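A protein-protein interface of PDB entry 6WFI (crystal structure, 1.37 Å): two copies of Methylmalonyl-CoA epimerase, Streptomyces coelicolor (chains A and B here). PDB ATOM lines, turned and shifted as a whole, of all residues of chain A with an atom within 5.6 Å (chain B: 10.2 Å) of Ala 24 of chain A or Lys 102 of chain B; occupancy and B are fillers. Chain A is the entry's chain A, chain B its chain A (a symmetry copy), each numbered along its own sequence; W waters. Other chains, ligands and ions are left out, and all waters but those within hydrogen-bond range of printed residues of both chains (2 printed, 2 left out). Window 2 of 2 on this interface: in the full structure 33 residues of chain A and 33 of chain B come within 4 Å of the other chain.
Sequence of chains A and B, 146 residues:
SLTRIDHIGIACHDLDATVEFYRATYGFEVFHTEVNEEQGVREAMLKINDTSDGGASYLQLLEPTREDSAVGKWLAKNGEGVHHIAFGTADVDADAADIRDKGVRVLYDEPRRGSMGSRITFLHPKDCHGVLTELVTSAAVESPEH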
ATOM      1  N   VAL A  19      11.940 -37.245 -12.006  1.00  0.00           N
ATOM      2  CA  VAL A  19      11.395 -37.725 -13.262  1.00  0.00           C
ATOM      3  C   VAL A  19      10.834 -36.561 -14.091  1.00  0.00           C
ATOM      4  O   VAL A  19      11.091 -36.446 -15.277  1.00  0.00           O
ATOM      5  CB  VAL A  19      10.338 -38.822 -13.016  1.00  0.00           C
ATOM      6  CG1 VAL A  19       9.447 -39.044 -14.199  1.00  0.00           C
ATOM      7  CG2 VAL A  19      11.002 -40.098 -12.582  1.00  0.00           C
ATOM      8  N   GLU A  20      10.021 -35.710 -13.441  1.00  0.00           N
ATOM      9  CA  GLU A  20       9.448 -34.562 -14.163  1.00  0.00           C
ATOM     10  C   GLU A  20      10.508 -33.568 -14.643  1.00  0.00           C
ATOM     11  O   GLU A  20      10.393 -33.040 -15.729  1.00  0.00           O
ATOM     12  CB  GLU A  20       8.420 -33.870 -13.251  1.00  0.00           C
ATOM     13  CG  GLU A  20       7.845 -32.618 -13.845  1.00  0.00           C
ATOM     14  CD  GLU A  20       7.159 -32.737 -15.178  1.00  0.00           C
ATOM     15  OE1 GLU A  20       6.826 -33.844 -15.658  1.00  0.00           O
ATOM     16  OE2 GLU A  20       6.973 -31.700 -15.848  1.00  0.00           O
ATOM     17  N   PHE A  21      11.536 -33.356 -13.840  1.00  0.00           N
ATOM     18  CA  PHE A  21      12.681 -32.544 -14.274  1.00  0.00           C
ATOM     19  C   PHE A  21      13.289 -33.028 -15.586  1.00  0.00           C
ATOM     20  O   PHE A  21      13.525 -32.285 -16.526  1.00  0.00           O
ATOM     21  CB  PHE A  21      13.731 -32.385 -13.169  1.00  0.00           C
ATOM     22  CG  PHE A  21      15.001 -31.764 -13.655  1.00  0.00           C
ATOM     23  CD1 PHE A  21      15.062 -30.398 -13.857  1.00  0.00           C
ATOM     24  CD2 PHE A  21      16.090 -32.531 -14.011  1.00  0.00           C
ATOM     25  CE1 PHE A  21      16.208 -29.843 -14.396  1.00  0.00           C
ATOM     26  CE2 PHE A  21      17.225 -31.936 -14.549  1.00  0.00           C
ATOM     27  CZ  PHE A  21      17.223 -30.621 -14.772  1.00  0.00           C
ATOM     28  N   TYR A  22      13.538 -34.357 -15.630  1.00  0.00           N
ATOM     29  CA  TYR A  22      14.179 -34.900 -16.847  1.00  0.00           C
ATOM     30  C   TYR A  22      13.212 -34.831 -18.052  1.00  0.00           C
ATOM     31  O   TYR A  22      13.664 -34.626 -19.156  1.00  0.00           O
ATOM     32  CB  TYR A  22      14.708 -36.317 -16.553  1.00  0.00           C
ATOM     33  CG  TYR A  22      16.050 -36.330 -15.851  1.00  0.00           C
ATOM     34  CD1 TYR A  22      16.175 -36.280 -14.492  1.00  0.00           C
ATOM     35  CD2 TYR A  22      17.208 -36.282 -16.600  1.00  0.00           C
ATOM     36  CE1 TYR A  22      17.392 -36.152 -13.855  1.00  0.00           C
ATOM     37  CE2 TYR A  22      18.440 -36.156 -16.015  1.00  0.00           C
ATOM     38  CZ  TYR A  22      18.540 -36.076 -14.640  1.00  0.00           C
ATOM     39  OH  TYR A  22      19.771 -35.892 -14.043  1.00  0.00           O
ATOM     40  N   ARG A  23      11.918 -35.061 -17.792  1.00  0.00           N
ATOM     41  CA  ARG A  23      10.921 -34.940 -18.879  1.00  0.00           C
ATOM     42  C   ARG A  23      10.829 -33.481 -19.397  1.00  0.00           C
ATOM     43  O   ARG A  23      10.933 -33.261 -20.585  1.00  0.00           O
ATOM     44  CB  ARG A  23       9.559 -35.434 -18.391  1.00  0.00           C
ATOM     45  CG  ARG A  23       8.532 -35.488 -19.517  1.00  0.00           C
ATOM     46  CD  ARG A  23       7.087 -35.319 -19.064  1.00  0.00           C
ATOM     47  NE  ARG A  23       6.870 -33.986 -18.531  1.00  0.00           N
ATOM     48  CZ  ARG A  23       6.789 -32.871 -19.260  1.00  0.00           C
ATOM     49  NH1 ARG A  23       6.834 -32.907 -20.578  1.00  0.00           N
ATOM     50  NH2 ARG A  23       6.710 -31.717 -18.645  1.00  0.00           N
ATOM     51  N   ALA A  24      10.636 -32.580 -18.459  1.00  0.00           N
ATOM     52  CA  ALA A  24      10.429 -31.164 -18.831  1.00  0.00           C
ATOM     53  C   ALA A  24      11.670 -30.596 -19.489  1.00  0.00           C
ATOM     54  O   ALA A  24      11.601 -29.789 -20.420  1.00  0.00           O
ATOM     55  CB  ALA A  24      10.052 -30.355 -17.643  1.00  0.00           C
ATOM     56  N   THR A  25      12.849 -30.943 -18.994  1.00  0.00           N
ATOM     57  CA  THR A  25      14.086 -30.284 -19.426  1.00  0.00           C
ATOM     58  C   THR A  25      14.613 -30.863 -20.725  1.00  0.00           C
ATOM     59  O   THR A  25      15.137 -30.157 -21.584  1.00  0.00           O
ATOM     60  CB  THR A  25      15.152 -30.303 -18.323  1.00  0.00           C
ATOM     61  OG1 THR A  25      14.578 -29.797 -17.110  1.00  0.00           O
ATOM     62  CG2 THR A  25      16.343 -29.437 -18.649  1.00  0.00           C
ATOM     63  N   TYR A  26      14.560 -32.203 -20.850  1.00  0.00           N
ATOM     64  CA  TYR A  26      15.198 -32.929 -21.959  1.00  0.00           C
ATOM     65  C   TYR A  26      14.239 -33.711 -22.837  1.00  0.00           C
ATOM     66  O   TYR A  26      14.710 -34.260 -23.852  1.00  0.00           O
ATOM     67  CB  TYR A  26      16.230 -33.893 -21.384  1.00  0.00           C
ATOM     68  CG  TYR A  26      17.173 -33.287 -20.362  1.00  0.00           C
ATOM     69  CD1 TYR A  26      18.022 -32.253 -20.674  1.00  0.00           C
ATOM     70  CD2 TYR A  26      17.200 -33.736 -19.071  1.00  0.00           C
ATOM     71  CE1 TYR A  26      18.886 -31.723 -19.716  1.00  0.00           C
ATOM     72  CE2 TYR A  26      18.069 -33.266 -18.110  1.00  0.00           C
ATOM     73  CZ  TYR A  26      18.953 -32.258 -18.441  1.00  0.00           C
ATOM     74  OH  TYR A  26      19.828 -31.767 -17.507  1.00  0.00           O
ATOM     75  N   GLY A  27      13.028 -33.871 -22.415  1.00  0.00           N
ATOM     76  CA  GLY A  27      12.016 -34.682 -23.135  1.00  0.00           C
ATOM     77  C   GLY A  27      12.180 -36.141 -22.844  1.00  0.00           C
ATOM     78  O   GLY A  27      11.570 -36.955 -23.602  1.00  0.00           O
ATOM     79  N   LEU B   2      18.436 -34.220 -27.234  1.00  0.00           N
ATOM     80  CA  LEU B   2      19.526 -35.046 -26.623  1.00  0.00           C
ATOM     81  C   LEU B   2      19.258 -36.505 -26.971  1.00  0.00           C
ATOM     82  O   LEU B   2      18.255 -37.090 -26.535  1.00  0.00           O
ATOM     83  CB  LEU B   2      19.557 -34.863 -25.115  1.00  0.00           C
ATOM     84  CG  LEU B   2      19.737 -33.433 -24.630  1.00  0.00           C
ATOM     85  CD1 LEU B   2      19.787 -33.443 -23.120  1.00  0.00           C
ATOM     86  CD2 LEU B   2      20.947 -32.730 -25.276  1.00  0.00           C
ATOM     87  N   ALA B  94      21.337 -25.005 -30.169  1.00  0.00           N
ATOM     88  CA  ALA B  94      19.877 -24.920 -30.109  1.00  0.00           C
ATOM     89  C   ALA B  94      19.351 -25.514 -28.825  1.00  0.00           C
ATOM     90  O   ALA B  94      18.422 -25.004 -28.166  1.00  0.00           O
ATOM     91  CB  ALA B  94      19.239 -25.600 -31.304  1.00  0.00           C
ATOM     92  N   ASP B  95      19.902 -26.674 -28.411  1.00  0.00           N
ATOM     93  CA  ASP B  95      19.404 -27.359 -27.194  1.00  0.00           C
ATOM     94  C   ASP B  95      19.794 -26.565 -25.978  1.00  0.00           C
ATOM     95  O   ASP B  95      18.949 -26.439 -25.056  1.00  0.00           O
ATOM     96  CB  ASP B  95      19.953 -28.771 -26.941  1.00  0.00           C
ATOM     97  CG  ASP B  95      19.185 -29.769 -27.760  1.00  0.00           C
ATOM     98  OD1 ASP B  95      17.945 -29.639 -27.891  1.00  0.00           O
ATOM     99  OD2 ASP B  95      19.868 -30.655 -28.281  1.00  0.00           O
ATOM    100  N   ALA B  96      20.934 -25.932 -25.949  1.00  0.00           N
ATOM    101  CA  ALA B  96      21.319 -25.063 -24.829  1.00  0.00           C
ATOM    102  C   ALA B  96      20.402 -23.838 -24.760  1.00  0.00           C
ATOM    103  O   ALA B  96      20.015 -23.463 -23.623  1.00  0.00           O
ATOM    104  CB  ALA B  96      22.746 -24.616 -25.028  1.00  0.00           C
ATOM    105  N   ALA B  97      19.999 -23.277 -25.877  1.00  0.00           N
ATOM    106  CA  ALA B  97      19.096 -22.098 -25.831  1.00  0.00           C
ATOM    107  C   ALA B  97      17.750 -22.532 -25.333  1.00  0.00           C
ATOM    108  O   ALA B  97      17.130 -21.834 -24.473  1.00  0.00           O
ATOM    109  CB  ALA B  97      18.986 -21.483 -27.176  1.00  0.00           C
ATOM    110  N   ASP B  98      17.261 -23.696 -25.728  1.00  0.00           N
ATOM    111  CA  ASP B  98      15.981 -24.158 -25.252  1.00  0.00           C
ATOM    112  C   ASP B  98      15.992 -24.390 -23.754  1.00  0.00           C
ATOM    113  O   ASP B  98      15.023 -24.112 -22.989  1.00  0.00           O
ATOM    114  CB  ASP B  98      15.541 -25.412 -26.004  1.00  0.00           C
ATOM    115  CG  ASP B  98      15.095 -25.103 -27.427  1.00  0.00           C
ATOM    116  OD1 ASP B  98      14.857 -23.892 -27.791  1.00  0.00           O
ATOM    117  OD2 ASP B  98      14.989 -26.102 -28.206  1.00  0.00           O
ATOM    118  N   ILE B  99      17.071 -24.947 -23.200  1.00  0.00           N
ATOM    119  CA  ILE B  99      17.198 -25.242 -21.769  1.00  0.00           C
ATOM    120  C   ILE B  99      17.379 -23.921 -20.989  1.00  0.00           C
ATOM    121  O   ILE B  99      16.759 -23.788 -19.908  1.00  0.00           O
ATOM    122  CB  ILE B  99      18.307 -26.288 -21.546  1.00  0.00           C
ATOM    123  CG1 ILE B  99      17.816 -27.619 -22.096  1.00  0.00           C
ATOM    124  CG2 ILE B  99      18.687 -26.388 -20.097  1.00  0.00           C
ATOM    125  CD1 ILE B  99      18.906 -28.670 -22.293  1.00  0.00           C
ATOM    126  N   ARG B 100      18.161 -23.009 -21.517  1.00  0.00           N
ATOM    127  CA  ARG B 100      18.256 -21.656 -20.904  1.00  0.00           C
ATOM    128  C   ARG B 100      16.848 -21.083 -20.746  1.00  0.00           C
ATOM    129  O   ARG B 100      16.558 -20.502 -19.678  1.00  0.00           O
ATOM    130  CB  ARG B 100      19.070 -20.783 -21.834  1.00  0.00           C
ATOM    131  CG  ARG B 100      19.062 -19.290 -21.436  1.00  0.00           C
ATOM    132  CD  ARG B 100      19.439 -18.417 -22.626  1.00  0.00           C
ATOM    133  NE  ARG B 100      18.355 -18.441 -23.609  1.00  0.00           N
ATOM    134  CZ  ARG B 100      18.463 -18.201 -24.903  1.00  0.00           C
ATOM    135  NH1 ARG B 100      19.623 -17.906 -25.426  1.00  0.00           N
ATOM    136  NH2 ARG B 100      17.408 -18.318 -25.692  1.00  0.00           N
ATOM    137  N   ASP B 101      15.994 -21.276 -21.726  1.00  0.00           N
ATOM    138  CA  ASP B 101      14.640 -20.689 -21.668  1.00  0.00           C
ATOM    139  C   ASP B 101      13.740 -21.400 -20.711  1.00  0.00           C
ATOM    140  O   ASP B 101      12.616 -20.894 -20.407  1.00  0.00           O
ATOM    141  CB  ASP B 101      14.059 -20.707 -23.049  1.00  0.00           C
ATOM    142  CG  ASP B 101      14.689 -19.660 -23.941  1.00  0.00           C
ATOM    143  OD1 ASP B 101      15.410 -18.787 -23.418  1.00  0.00           O
ATOM    144  OD2 ASP B 101      14.410 -19.778 -25.129  1.00  0.00           O
ATOM    145  N   LYS B 102      14.177 -22.479 -20.056  1.00  0.00           N
ATOM    146  CA  LYS B 102      13.450 -23.139 -18.961  1.00  0.00           C
ATOM    147  C   LYS B 102      13.948 -22.673 -17.602  1.00  0.00           C
ATOM    148  O   LYS B 102      13.418 -23.095 -16.567  1.00  0.00           O
ATOM    149  CB  LYS B 102      13.591 -24.665 -19.085  1.00  0.00           C
ATOM    150  CG  LYS B 102      12.995 -25.152 -20.356  1.00  0.00           C
ATOM    151  CD  LYS B 102      13.268 -26.676 -20.512  1.00  0.00           C
ATOM    152  CE  LYS B 102      13.063 -27.167 -21.902  1.00  0.00           C
ATOM    153  NZ  LYS B 102      11.625 -27.229 -22.055  1.00  0.00           N
ATOM    154  N   GLY B 103      14.974 -21.835 -17.538  1.00  0.00           N
ATOM    155  CA  GLY B 103      15.483 -21.335 -16.255  1.00  0.00           C
ATOM    156  C   GLY B 103      16.594 -22.137 -15.630  1.00  0.00           C
ATOM    157  O   GLY B 103      17.089 -21.816 -14.558  1.00  0.00           O
ATOM    158  N   VAL B 104      17.047 -23.196 -16.336  1.00  0.00           N
ATOM    159  CA  VAL B 104      18.251 -23.960 -15.928  1.00  0.00           C
ATOM    160  C   VAL B 104      19.460 -23.117 -16.345  1.00  0.00           C
ATOM    161  O   VAL B 104      19.535 -22.692 -17.491  1.00  0.00           O
ATOM    162  CB  VAL B 104      18.219 -25.338 -16.615  1.00  0.00           C
ATOM    163  CG1 VAL B 104      19.548 -26.065 -16.364  1.00  0.00           C
ATOM    164  CG2 VAL B 104      17.042 -26.162 -16.129  1.00  0.00           C
ATOM    165  N   ARG B 105      20.397 -22.910 -15.425  1.00  0.00           N
ATOM    166  CA  ARG B 105      21.568 -22.123 -15.733  1.00  0.00           C
ATOM    167  C   ARG B 105      22.469 -22.822 -16.737  1.00  0.00           C
ATOM    168  O   ARG B 105      23.025 -23.901 -16.376  1.00  0.00           O
ATOM    169  CB  ARG B 105      22.332 -21.732 -14.477  1.00  0.00           C
ATOM    170  CG  ARG B 105      21.626 -20.601 -13.695  1.00  0.00           C
ATOM    171  CD  ARG B 105      22.270 -20.442 -12.352  1.00  0.00           C
ATOM    172  NE  ARG B 105      21.902 -21.510 -11.444  1.00  0.00           N
ATOM    173  CZ  ARG B 105      22.368 -21.678 -10.238  1.00  0.00           C
ATOM    174  NH1 ARG B 105      23.315 -20.889  -9.774  1.00  0.00           N
ATOM    175  NH2 ARG B 105      21.880 -22.649  -9.473  1.00  0.00           N
ATOM    176  N   VAL B 106      22.721 -22.235 -17.868  1.00  0.00           N
ATOM    177  CA  VAL B 106      23.688 -22.697 -18.882  1.00  0.00           C
ATOM    178  C   VAL B 106      24.970 -21.970 -18.642  1.00  0.00           C
ATOM    179  O   VAL B 106      24.973 -20.690 -18.700  1.00  0.00           O
ATOM    180  CB  VAL B 106      23.122 -22.467 -20.266  1.00  0.00           C
ATOM    181  CG1 VAL B 106      24.164 -22.858 -21.308  1.00  0.00           C
ATOM    182  CG2 VAL B 106      21.852 -23.203 -20.485  1.00  0.00           C
ATOM    183  N   LEU B 123      25.344 -27.436 -17.679  1.00  0.00           N
ATOM    184  CA  LEU B 123      24.188 -26.973 -16.902  1.00  0.00           C
ATOM    185  C   LEU B 123      24.561 -27.033 -15.455  1.00  0.00           C
ATOM    186  O   LEU B 123      25.163 -28.011 -14.958  1.00  0.00           O
ATOM    187  CB  LEU B 123      23.001 -27.855 -17.172  1.00  0.00           C
ATOM    188  CG  LEU B 123      22.654 -28.098 -18.629  1.00  0.00           C
ATOM    189  CD1 LEU B 123      21.456 -28.990 -18.790  1.00  0.00           C
ATOM    190  CD2 LEU B 123      22.429 -26.771 -19.384  1.00  0.00           C
ATOM    191  N   ASP B 127      20.807 -26.832 -10.452  1.00  0.00           N
ATOM    192  CA  ASP B 127      19.570 -26.778 -11.215  1.00  0.00           C
ATOM    193  C   ASP B 127      19.182 -28.138 -11.809  1.00  0.00           C
ATOM    194  O   ASP B 127      18.133 -28.259 -12.427  1.00  0.00           O
ATOM    195  CB  ASP B 127      19.615 -25.738 -12.328  1.00  0.00           C
ATOM    196  CG  ASP B 127      19.810 -24.300 -11.856  1.00  0.00           C
ATOM    197  OD1 ASP B 127      19.595 -24.067 -10.617  1.00  0.00           O
ATOM    198  OD2 ASP B 127      20.190 -23.484 -12.673  1.00  0.00           O
ATOM    199  N   CYS B 128      20.009 -29.156 -11.570  1.00  0.00           N
ATOM    200  CA  CYS B 128      19.841 -30.472 -12.206  1.00  0.00           C
ATOM    201  C   CYS B 128      19.828 -31.518 -11.127  1.00  0.00           C
ATOM    202  O   CYS B 128      20.342 -32.658 -11.330  1.00  0.00           O
ATOM    203  CB  CYS B 128      20.942 -30.781 -13.215  1.00  0.00           C
ATOM    204  SG  CYS B 128      21.038 -29.611 -14.604  1.00  0.00           S
ATOM    205  N   HIS B 129      19.268 -31.275  -9.958  1.00  0.00           N
ATOM    206  CA  HIS B 129      19.173 -32.260  -8.867  1.00  0.00           C
ATOM    207  C   HIS B 129      20.556 -32.813  -8.580  1.00  0.00           C
ATOM    208  O   HIS B 129      20.693 -34.038  -8.315  1.00  0.00           O
ATOM    209  CB  HIS B 129      18.066 -33.282  -9.175  1.00  0.00           C
ATOM    210  CG  HIS B 129      16.696 -32.718  -9.127  1.00  0.00           C
ATOM    211  ND1 HIS B 129      16.119 -32.570  -7.860  1.00  0.00           N
ATOM    212  CD2 HIS B 129      15.891 -32.213 -10.035  1.00  0.00           C
ATOM    213  CE1 HIS B 129      14.922 -32.029  -8.092  1.00  0.00           C
ATOM    214  NE2 HIS B 129      14.687 -31.836  -9.391  1.00  0.00           N
ATOM    215  N   LEU B 135      26.316 -30.896 -22.264  1.00  0.00           N
ATOM    216  CA  LEU B 135      25.715 -31.105 -23.577  1.00  0.00           C
ATOM    217  C   LEU B 135      26.823 -31.027 -24.614  1.00  0.00           C
ATOM    218  O   LEU B 135      27.644 -30.107 -24.518  1.00  0.00           O
ATOM    219  CB  LEU B 135      24.652 -30.070 -23.891  1.00  0.00           C
ATOM    220  CG  LEU B 135      23.653 -29.800 -22.767  1.00  0.00           C
ATOM    221  CD1 LEU B 135      22.650 -28.703 -23.226  1.00  0.00           C
ATOM    222  CD2 LEU B 135      22.895 -31.013 -22.322  1.00  0.00           C
HETATM  223  O   HOH W   1       9.684 -27.161 -19.924  1.00  0.00           O
HETATM  224  O   HOH W   2      19.604 -35.399 -11.452  1.00  0.00           O
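Water W2 lies within hydrogen-bond range of the side-chain hydroxyl (OH) of Tyr 22 of chain A and the backbone carbonyl oxygen (O) of Cys 128 of chain B.
Water W1 lies within hydrogen-bond range of the side-chain amino group of Lys 102 of chain B and the backbone carbonyl oxygen of Ala 24 of chain A.
No residue of chain B comes within 4 Å of Glu 20 of chain A.
Printed residues of chain B within 4 Å of Ala 24 of chain A: Lys 102 (3.0 Å).
Of chain B, only Ile 99 (3.7 Å) and Lys 102 (3.7 Å) come within 4 Å of Thr 25 of chain A.
Of the printed residues of chain A, Ile 99 of chain B touches Thr 25 and Tyr 26.
Arg 100 of chain B touches none of the printed residues of chain A.
Lys 102 of chain B touches just these residues of chain A: Ala 24 and Thr 25.
Printed residues of chain A within 4 Å of Asp 127 of chain B: Phe 21 (3.2 Å).
Of the printed residues of chain A, Cys 128 of chain B touches Phe 21 and Tyr 26.
The nearest residue of chain B that does not touch Ala 24 of chain A is Ile 99 of chain B (6.8 Å).
The nearest residue of chain A that does not touch Lys 102 of chain B is Tyr 26 of chain A (5.4 Å).
The nearest printed residue of chain A that does not touch His 129 of chain B is Tyr 22 of chain A (5.5 Å).
No position is printed for both chains.
Of the 19 printed residues of chain B, 7 touch a printed residue of chain A.
Printed residues of chain B that touch a printed residue of chain A: Leu 2, Ile 99, Lys 102, Leu 123, Asp 127, Cys 128 and His 129.
Printed residues of chain A that touch a printed residue of chain B: Phe 21, Ala 24, Thr 25 and Tyr 26.
Hydrophobic or aromatic side chains of chain A that line the printed part of chain B: Phe 21 and Tyr 26.
OG1 of Thr 25 of chain A is in hydrogen-bond range of O of Phe 21 of chain A (2.8 Å).
NE of Arg 105 of chain B is in salt-bridge range of OD2 of Asp 127 of chain B (2.9 Å).
CE1 of Phe 21 of chain A touches O of Asp 127 of chain B (3.2 Å).
Phe 21 of chain A touches Cys 128 of chain B.
His 129 of chain B touches Phe 21 of chain A (CD2 to CG, 3.8 Å).
Thr 25 of chain A touches Ile 99 of chain B (O to CG1, 3.7 Å).
O of Thr 25 of chain A touches CE of Lys 102 of chain B, at 3.7 Å.
Tyr 26 of chain A touches Leu 2 of chain B.
Tyr 26 of chain A touches Ile 99 of chain B.
Leu 123 of chain B touches Tyr 26 of chain A.
SG of Cys 128 of chain B touches OH of Tyr 26 of chain A, 3.8 Å away.
The backbone carbonyl oxygen (O) of Ala 24 of chain A is in hydrogen-bond range of the side-chain amino group (NZ) of Lys 102 of chain B, 3.0 Å away.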
